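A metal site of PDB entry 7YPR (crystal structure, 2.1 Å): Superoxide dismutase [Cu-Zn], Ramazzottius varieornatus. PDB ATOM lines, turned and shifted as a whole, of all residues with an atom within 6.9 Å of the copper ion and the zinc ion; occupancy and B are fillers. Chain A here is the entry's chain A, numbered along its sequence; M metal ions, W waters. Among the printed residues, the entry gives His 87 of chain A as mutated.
The zinc ion is bound by OD1 of Asp 124. ND1 of His 121 is bound to the zinc ion. A ring nitrogen (ND1) of His 104 is bound to the zinc ion (2.2 Å). ND1 of His 112 binds the zinc ion, at 2.2 Å. The zinc ion has four donor atoms within binding distance.
The nearest printed residue that does not touch the copper ion is Asn 179 (4.4 Å).
NE2 of His 112 is in hydrogen-bond range of OD1 of Asp 166 (2.7 Å). The backbone NH (N) of Val 160 lies within hydrogen-bond range of the backbone carbonyl oxygen (O) of His 85, 2.7 Å away. The side-chain carboxylate of Asp 124 is in hydrogen-bond range of the backbone NH of Gly 113 (2.9 Å). The backbone carbonyl oxygen (O) of Gly 183 lies within hydrogen-bond range of a ring nitrogen (ND1) of His 162 (3.1 Å). The backbone NH (N) of Gly 180 sits close to a ring nitrogen (NE2) of His 112, at 3.3 Å. The backbone NH of His 162 lies within hydrogen-bond range of the backbone carbonyl oxygen of Gly 83, at 2.8 Å. A ring nitrogen (NE2) of His 85 sits at hydrogen-bond distance from the side-chain carboxylate (OD2) of Asp 166 (2.8 Å). O of Asp 124 sits at hydrogen-bond distance from NH2 of Arg 120 (3.2 Å).
The copper ion is bound by a ring nitrogen (NE2) of His 104. NE2 of His 162 is bound to the copper ion, at 2.0 Å. The copper ion is bound by ND1 of His 85 (2.1 Å).
Of the 29 residues printed, 4 come within 4 Å of the zinc ion. The nearest printed residue that does not touch the zinc ion is Val 178 (4.02 Å).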
ATOM      1  N   GLY A  83      11.434  22.862   1.070  1.00  0.00           N
ATOM      2  CA  GLY A  83      10.568  22.252   0.081  1.00  0.00           C
ATOM      3  C   GLY A  83       9.096  22.415   0.422  1.00  0.00           C
ATOM      4  O   GLY A  83       8.691  22.397   1.599  1.00  0.00           O
ATOM      5  N   LEU A  84       8.288  22.593  -0.612  1.00  0.00           N
ATOM      6  CA  LEU A  84       6.860  22.837  -0.514  1.00  0.00           C
ATOM      7  C   LEU A  84       6.176  21.839  -1.444  1.00  0.00           C
ATOM      8  O   LEU A  84       6.265  21.964  -2.664  1.00  0.00           O
ATOM      9  CB  LEU A  84       6.521  24.278  -0.924  1.00  0.00           C
ATOM     10  CG  LEU A  84       5.044  24.624  -0.967  1.00  0.00           C
ATOM     11  CD1 LEU A  84       4.523  24.864   0.452  1.00  0.00           C
ATOM     12  CD2 LEU A  84       4.795  25.840  -1.842  1.00  0.00           C
ATOM     13  N   HIS A  85       5.509  20.840  -0.864  1.00  0.00           N
ATOM     14  CA  HIS A  85       5.018  19.712  -1.654  1.00  0.00           C
ATOM     15  C   HIS A  85       3.596  19.380  -1.237  1.00  0.00           C
ATOM     16  O   HIS A  85       3.214  19.534  -0.072  1.00  0.00           O
ATOM     17  CB  HIS A  85       5.903  18.450  -1.467  1.00  0.00           C
ATOM     18  CG  HIS A  85       7.346  18.653  -1.813  1.00  0.00           C
ATOM     19  ND1 HIS A  85       8.368  18.047  -1.125  1.00  0.00           N
ATOM     20  CD2 HIS A  85       7.938  19.396  -2.789  1.00  0.00           C
ATOM     21  CE1 HIS A  85       9.530  18.408  -1.636  1.00  0.00           C
ATOM     22  NE2 HIS A  85       9.298  19.223  -2.652  1.00  0.00           N
ATOM     23  N   ILE A  86       2.810  18.934  -2.204  1.00  0.00           N
ATOM     24  CA  ILE A  86       1.486  18.385  -1.938  1.00  0.00           C
ATOM     25  C   ILE A  86       1.583  16.870  -1.895  1.00  0.00           C
ATOM     26  O   ILE A  86       2.017  16.229  -2.863  1.00  0.00           O
ATOM     27  CB  ILE A  86       0.479  18.839  -2.992  1.00  0.00           C
ATOM     28  CG1 ILE A  86       0.431  20.376  -2.989  1.00  0.00           C
ATOM     29  CG2 ILE A  86      -0.902  18.202  -2.719  1.00  0.00           C
ATOM     30  CD1 ILE A  86      -0.353  20.936  -4.170  1.00  0.00           C
ATOM     31  N   HIS A  87       1.177  16.286  -0.784  1.00  0.00           N
ATOM     32  CA  HIS A  87       1.300  14.856  -0.554  1.00  0.00           C
ATOM     33  C   HIS A  87       0.092  14.127  -1.133  1.00  0.00           C
ATOM     34  O   HIS A  87      -0.976  14.697  -1.344  1.00  0.00           O
ATOM     35  CB  HIS A  87       1.435  14.589   0.954  1.00  0.00           C
ATOM     36  CG  HIS A  87       1.969  13.234   1.274  1.00  0.00           C
ATOM     37  ND1 HIS A  87       1.167  12.108   1.294  1.00  0.00           N
ATOM     38  CD2 HIS A  87       3.224  12.810   1.570  1.00  0.00           C
ATOM     39  CE1 HIS A  87       1.905  11.051   1.598  1.00  0.00           C
ATOM     40  NE2 HIS A  87       3.150  11.450   1.777  1.00  0.00           N
ATOM     41  N   GLY A 103       3.905   8.966  -0.553  1.00  0.00           N
ATOM     42  CA  GLY A 103       4.707   9.995  -1.212  1.00  0.00           C
ATOM     43  C   GLY A 103       3.902  11.137  -1.825  1.00  0.00           C
ATOM     44  O   GLY A 103       2.701  11.309  -1.578  1.00  0.00           O
ATOM     45  N   HIS A 104       4.585  11.935  -2.651  1.00  0.00           N
ATOM     46  CA  HIS A 104       3.989  13.156  -3.203  1.00  0.00           C
ATOM     47  C   HIS A 104       2.837  12.821  -4.147  1.00  0.00           C
ATOM     48  O   HIS A 104       2.815  11.762  -4.777  1.00  0.00           O
ATOM     49  CB  HIS A 104       5.031  13.985  -3.968  1.00  0.00           C
ATOM     50  CG  HIS A 104       6.131  14.512  -3.090  1.00  0.00           C
ATOM     51  ND1 HIS A 104       7.342  14.916  -3.586  1.00  0.00           N
ATOM     52  CD2 HIS A 104       6.190  14.692  -1.755  1.00  0.00           C
ATOM     53  CE1 HIS A 104       8.112  15.336  -2.598  1.00  0.00           C
ATOM     54  NE2 HIS A 104       7.427  15.211  -1.473  1.00  0.00           N
ATOM     55  N   LEU A 105       1.898  13.762  -4.240  1.00  0.00           N
ATOM     56  CA  LEU A 105       0.754  13.595  -5.133  1.00  0.00           C
ATOM     57  C   LEU A 105       1.238  13.340  -6.565  1.00  0.00           C
ATOM     58  O   LEU A 105       1.910  14.190  -7.149  1.00  0.00           O
ATOM     59  CB  LEU A 105      -0.120  14.852  -5.075  1.00  0.00           C
ATOM     60  CG  LEU A 105      -1.399  14.850  -5.899  1.00  0.00           C
ATOM     61  CD1 LEU A 105      -2.343  13.698  -5.460  1.00  0.00           C
ATOM     62  CD2 LEU A 105      -2.090  16.193  -5.842  1.00  0.00           C
ATOM     63  N   ASN A 106       0.923  12.166  -7.113  1.00  0.00           N
ATOM     64  CA  ASN A 106       1.583  11.776  -8.357  1.00  0.00           C
ATOM     65  C   ASN A 106       0.663  10.954  -9.266  1.00  0.00           C
ATOM     66  O   ASN A 106       0.995   9.817  -9.611  1.00  0.00           O
ATOM     67  CB  ASN A 106       2.873  11.012  -8.024  1.00  0.00           C
ATOM     68  CG  ASN A 106       3.715  10.719  -9.256  1.00  0.00           C
ATOM     69  OD1 ASN A 106       3.563  11.360 -10.294  1.00  0.00           O
ATOM     70  ND2 ASN A 106       4.598   9.733  -9.147  1.00  0.00           N
ATOM     71  N   SER A 111       8.553  11.095 -12.145  1.00  0.00           N
ATOM     72  CA  SER A 111       9.537  11.185 -11.068  1.00  0.00           C
ATOM     73  C   SER A 111       9.589  12.609 -10.489  1.00  0.00           C
ATOM     74  O   SER A 111       9.079  13.560 -11.067  1.00  0.00           O
ATOM     75  CB  SER A 111      10.907  10.766 -11.583  1.00  0.00           C
ATOM     76  OG  SER A 111      11.164  11.402 -12.810  1.00  0.00           O
ATOM     77  N   HIS A 112      10.228  12.735  -9.332  1.00  0.00           N
ATOM     78  CA  HIS A 112      10.276  14.012  -8.654  1.00  0.00           C
ATOM     79  C   HIS A 112      11.060  15.025  -9.482  1.00  0.00           C
ATOM     80  O   HIS A 112      12.147  14.718  -9.982  1.00  0.00           O
ATOM     81  CB  HIS A 112      10.893  13.861  -7.256  1.00  0.00           C
ATOM     82  CG  HIS A 112      11.033  15.157  -6.518  1.00  0.00           C
ATOM     83  ND1 HIS A 112       9.984  15.758  -5.852  1.00  0.00           N
ATOM     84  CD2 HIS A 112      12.095  15.998  -6.375  1.00  0.00           C
ATOM     85  CE1 HIS A 112      10.387  16.902  -5.317  1.00  0.00           C
ATOM     86  NE2 HIS A 112      11.658  17.070  -5.620  1.00  0.00           N
ATOM     87  N   GLY A 113      10.522  16.236  -9.631  1.00  0.00           N
ATOM     88  CA  GLY A 113      11.229  17.265 -10.360  1.00  0.00           C
ATOM     89  C   GLY A 113      11.016  18.656  -9.809  1.00  0.00           C
ATOM     90  O   GLY A 113      10.390  18.844  -8.763  1.00  0.00           O
ATOM     91  N   ARG A 120       7.834  15.885 -13.371  1.00  0.00           N
ATOM     92  CA  ARG A 120       7.588  16.257 -11.983  1.00  0.00           C
ATOM     93  C   ARG A 120       6.339  15.556 -11.487  1.00  0.00           C
ATOM     94  O   ARG A 120       5.506  15.100 -12.270  1.00  0.00           O
ATOM     95  CB  ARG A 120       7.426  17.777 -11.827  1.00  0.00           C
ATOM     96  CG  ARG A 120       6.400  18.368 -12.794  1.00  0.00           C
ATOM     97  CD  ARG A 120       6.056  19.794 -12.411  1.00  0.00           C
ATOM     98  NE  ARG A 120       5.080  19.852 -11.322  1.00  0.00           N
ATOM     99  CZ  ARG A 120       4.433  20.947 -10.965  1.00  0.00           C
ATOM    100  NH1 ARG A 120       4.659  22.112 -11.559  1.00  0.00           N
ATOM    101  NH2 ARG A 120       3.553  20.889  -9.958  1.00  0.00           N
ATOM    102  N   HIS A 121       6.226  15.460 -10.158  1.00  0.00           N
ATOM    103  CA  HIS A 121       4.948  15.098  -9.576  1.00  0.00           C
ATOM    104  C   HIS A 121       4.004  16.289  -9.634  1.00  0.00           C
ATOM    105  O   HIS A 121       4.434  17.437  -9.640  1.00  0.00           O
ATOM    106  CB  HIS A 121       5.147  14.682  -8.118  1.00  0.00           C
ATOM    107  CG  HIS A 121       6.104  13.546  -7.946  1.00  0.00           C
ATOM    108  ND1 HIS A 121       6.942  13.458  -6.863  1.00  0.00           N
ATOM    109  CD2 HIS A 121       6.329  12.442  -8.695  1.00  0.00           C
ATOM    110  CE1 HIS A 121       7.669  12.355  -6.958  1.00  0.00           C
ATOM    111  NE2 HIS A 121       7.308  11.718  -8.058  1.00  0.00           N
ATOM    112  N   VAL A 122       2.704  16.016  -9.667  1.00  0.00           N
ATOM    113  CA  VAL A 122       1.754  17.118  -9.496  1.00  0.00           C
ATOM    114  C   VAL A 122       2.063  17.905  -8.232  1.00  0.00           C
ATOM    115  O   VAL A 122       2.042  19.140  -8.225  1.00  0.00           O
ATOM    116  CB  VAL A 122       0.306  16.592  -9.493  1.00  0.00           C
ATOM    117  CG1 VAL A 122      -0.645  17.669  -8.970  1.00  0.00           C
ATOM    118  CG2 VAL A 122      -0.105  16.178 -10.901  1.00  0.00           C
ATOM    119  N   GLY A 123       2.410  17.205  -7.157  1.00  0.00           N
ATOM    120  CA  GLY A 123       2.661  17.901  -5.921  1.00  0.00           C
ATOM    121  C   GLY A 123       3.983  18.632  -5.783  1.00  0.00           C
ATOM    122  O   GLY A 123       4.274  19.110  -4.687  1.00  0.00           O
ATOM    123  N   ASP A 124       4.793  18.756  -6.844  1.00  0.00           N
ATOM    124  CA  ASP A 124       6.139  19.333  -6.734  1.00  0.00           C
ATOM    125  C   ASP A 124       6.059  20.857  -6.955  1.00  0.00           C
ATOM    126  O   ASP A 124       6.078  21.325  -8.089  1.00  0.00           O
ATOM    127  CB  ASP A 124       7.088  18.706  -7.740  1.00  0.00           C
ATOM    128  CG  ASP A 124       7.420  17.247  -7.421  1.00  0.00           C
ATOM    129  OD1 ASP A 124       7.088  16.768  -6.315  1.00  0.00           O
ATOM    130  OD2 ASP A 124       8.023  16.572  -8.293  1.00  0.00           O
ATOM    131  N   LEU A 125       6.025  21.624  -5.858  1.00  0.00           N
ATOM    132  CA  LEU A 125       5.906  23.075  -5.940  1.00  0.00           C
ATOM    133  C   LEU A 125       7.222  23.791  -5.617  1.00  0.00           C
ATOM    134  O   LEU A 125       7.243  25.016  -5.515  1.00  0.00           O
ATOM    135  CB  LEU A 125       4.782  23.583  -5.017  1.00  0.00           C
ATOM    136  CG  LEU A 125       3.386  23.028  -5.345  1.00  0.00           C
ATOM    137  CD1 LEU A 125       2.290  23.621  -4.460  1.00  0.00           C
ATOM    138  CD2 LEU A 125       3.050  23.280  -6.801  1.00  0.00           C
ATOM    139  N   VAL A 160       2.805  20.215   2.516  1.00  0.00           N
ATOM    140  CA  VAL A 160       3.892  19.982   3.449  1.00  0.00           C
ATOM    141  C   VAL A 160       4.954  21.066   3.271  1.00  0.00           C
ATOM    142  O   VAL A 160       5.302  21.409   2.136  1.00  0.00           O
ATOM    143  CB  VAL A 160       4.536  18.589   3.211  1.00  0.00           C
ATOM    144  CG1 VAL A 160       5.795  18.400   4.056  1.00  0.00           C
ATOM    145  CG2 VAL A 160       3.544  17.486   3.523  1.00  0.00           C
ATOM    146  N   HIS A 162       8.853  21.356   4.242  1.00  0.00           N
ATOM    147  CA  HIS A 162       9.889  20.439   4.662  1.00  0.00           C
ATOM    148  C   HIS A 162      10.962  21.125   5.496  1.00  0.00           C
ATOM    149  O   HIS A 162      11.147  22.345   5.461  1.00  0.00           O
ATOM    150  CB  HIS A 162      10.541  19.777   3.454  1.00  0.00           C
ATOM    151  CG  HIS A 162       9.793  18.591   2.936  1.00  0.00           C
ATOM    152  ND1 HIS A 162       9.800  17.372   3.566  1.00  0.00           N
ATOM    153  CD2 HIS A 162       9.042  18.421   1.819  1.00  0.00           C
ATOM    154  CE1 HIS A 162       9.083  16.503   2.879  1.00  0.00           C
ATOM    155  NE2 HIS A 162       8.600  17.115   1.810  1.00  0.00           N
ATOM    156  N   ASP A 166      14.330  21.428  -1.209  1.00  0.00           N
ATOM    157  CA  ASP A 166      14.080  20.470  -2.281  1.00  0.00           C
ATOM    158  C   ASP A 166      15.221  20.591  -3.293  1.00  0.00           C
ATOM    159  O   ASP A 166      15.487  21.691  -3.791  1.00  0.00           O
ATOM    160  CB  ASP A 166      12.742  20.832  -2.902  1.00  0.00           C
ATOM    161  CG  ASP A 166      12.320  19.920  -4.035  1.00  0.00           C
ATOM    162  OD1 ASP A 166      13.059  19.001  -4.430  1.00  0.00           O
ATOM    163  OD2 ASP A 166      11.199  20.150  -4.549  1.00  0.00           O
ATOM    164  N   SER A 176      16.632  11.566  -4.309  1.00  0.00           N
ATOM    165  CA  SER A 176      16.510  12.831  -5.025  1.00  0.00           C
ATOM    166  C   SER A 176      15.347  12.792  -6.011  1.00  0.00           C
ATOM    167  O   SER A 176      14.561  13.742  -6.104  1.00  0.00           O
ATOM    168  CB  SER A 176      17.821  13.155  -5.761  1.00  0.00           C
ATOM    169  OG  SER A 176      18.790  13.693  -4.890  1.00  0.00           O
ATOM    170  N   LYS A 177      15.219  11.695  -6.762  1.00  0.00           N
ATOM    171  CA  LYS A 177      14.121  11.564  -7.727  1.00  0.00           C
ATOM    172  C   LYS A 177      12.847  11.011  -7.121  1.00  0.00           C
ATOM    173  O   LYS A 177      11.866  10.811  -7.837  1.00  0.00           O
ATOM    174  CB  LYS A 177      14.554  10.684  -8.911  1.00  0.00           C
ATOM    175  CG  LYS A 177      15.757  11.224  -9.647  1.00  0.00           C
ATOM    176  CD  LYS A 177      15.319  12.326 -10.590  1.00  0.00           C
ATOM    177  CE  LYS A 177      16.105  12.309 -11.896  1.00  0.00           C
ATOM    178  NZ  LYS A 177      16.061  13.664 -12.523  1.00  0.00           N
ATOM    179  N   VAL A 178      12.834  10.749  -5.811  1.00  0.00           N
ATOM    180  CA  VAL A 178      11.616  10.363  -5.114  1.00  0.00           C
ATOM    181  C   VAL A 178      10.931  11.576  -4.483  1.00  0.00           C
ATOM    182  O   VAL A 178       9.721  11.756  -4.634  1.00  0.00           O
ATOM    183  CB  VAL A 178      11.951   9.289  -4.062  1.00  0.00           C
ATOM    184  CG1 VAL A 178      10.728   8.964  -3.212  1.00  0.00           C
ATOM    185  CG2 VAL A 178      12.454   8.042  -4.763  1.00  0.00           C
ATOM    186  N   ASN A 179      11.700  12.442  -3.849  1.00  0.00           N
ATOM    187  CA  ASN A 179      11.099  13.583  -3.181  1.00  0.00           C
ATOM    188  C   ASN A 179      12.044  14.777  -3.040  1.00  0.00           C
ATOM    189  O   ASN A 179      11.727  15.683  -2.256  1.00  0.00           O
ATOM    190  CB  ASN A 179      10.602  13.183  -1.780  1.00  0.00           C
ATOM    191  CG  ASN A 179      11.661  12.467  -0.984  1.00  0.00           C
ATOM    192  OD1 ASN A 179      12.834  12.883  -0.953  1.00  0.00           O
ATOM    193  ND2 ASN A 179      11.259  11.408  -0.300  1.00  0.00           N
ATOM    194  N   GLY A 180      13.169  14.811  -3.734  1.00  0.00           N
ATOM    195  CA  GLY A 180      14.061  15.949  -3.612  1.00  0.00           C
ATOM    196  C   GLY A 180      14.882  15.993  -2.347  1.00  0.00           C
ATOM    197  O   GLY A 180      15.588  16.974  -2.121  1.00  0.00           O
ATOM    198  N   ALA A 182      14.327  16.502   0.796  1.00  0.00           N
ATOM    199  CA  ALA A 182      14.133  17.708   1.585  1.00  0.00           C
ATOM    200  C   ALA A 182      13.959  17.421   3.065  1.00  0.00           C
ATOM    201  O   ALA A 182      13.698  18.349   3.828  1.00  0.00           O
ATOM    202  CB  ALA A 182      12.950  18.495   1.049  1.00  0.00           C
ATOM    203  N   GLY A 183      14.099  16.160   3.495  1.00  0.00           N
ATOM    204  CA  GLY A 183      14.075  15.857   4.921  1.00  0.00           C
ATOM    205  C   GLY A 183      12.693  15.701   5.503  1.00  0.00           C
ATOM    206  O   GLY A 183      11.753  15.324   4.802  1.00  0.00           O
ATOM    207  N   ARG A 185       9.221  16.888   7.962  1.00  0.00           N
ATOM    208  CA  ARG A 185       8.171  17.880   7.846  1.00  0.00           C
ATOM    209  C   ARG A 185       8.268  18.835   9.026  1.00  0.00           C
ATOM    210  O   ARG A 185       8.439  18.402  10.165  1.00  0.00           O
ATOM    211  CB  ARG A 185       6.796  17.230   7.787  1.00  0.00           C
ATOM    212  CG  ARG A 185       6.726  16.089   6.778  1.00  0.00           C
ATOM    213  CD  ARG A 185       5.442  15.291   6.923  1.00  0.00           C
ATOM    214  NE  ARG A 185       5.617  13.951   6.394  1.00  0.00           N
ATOM    215  CZ  ARG A 185       5.805  12.865   7.127  1.00  0.00           C
ATOM    216  NH1 ARG A 185       5.804  12.912   8.447  1.00  0.00           N
ATOM    217  NH2 ARG A 185       6.000  11.702   6.514  1.00  0.00           N
HETATM  218 CU    CU M   1       7.973  16.355   0.021  1.00  0.00          CU
HETATM  219 ZN    ZN M   2       7.833  15.123  -5.744  1.00  0.00          ZN
HETATM  220  O   HOH W   1       6.008  14.865   1.551  1.00  0.00           O
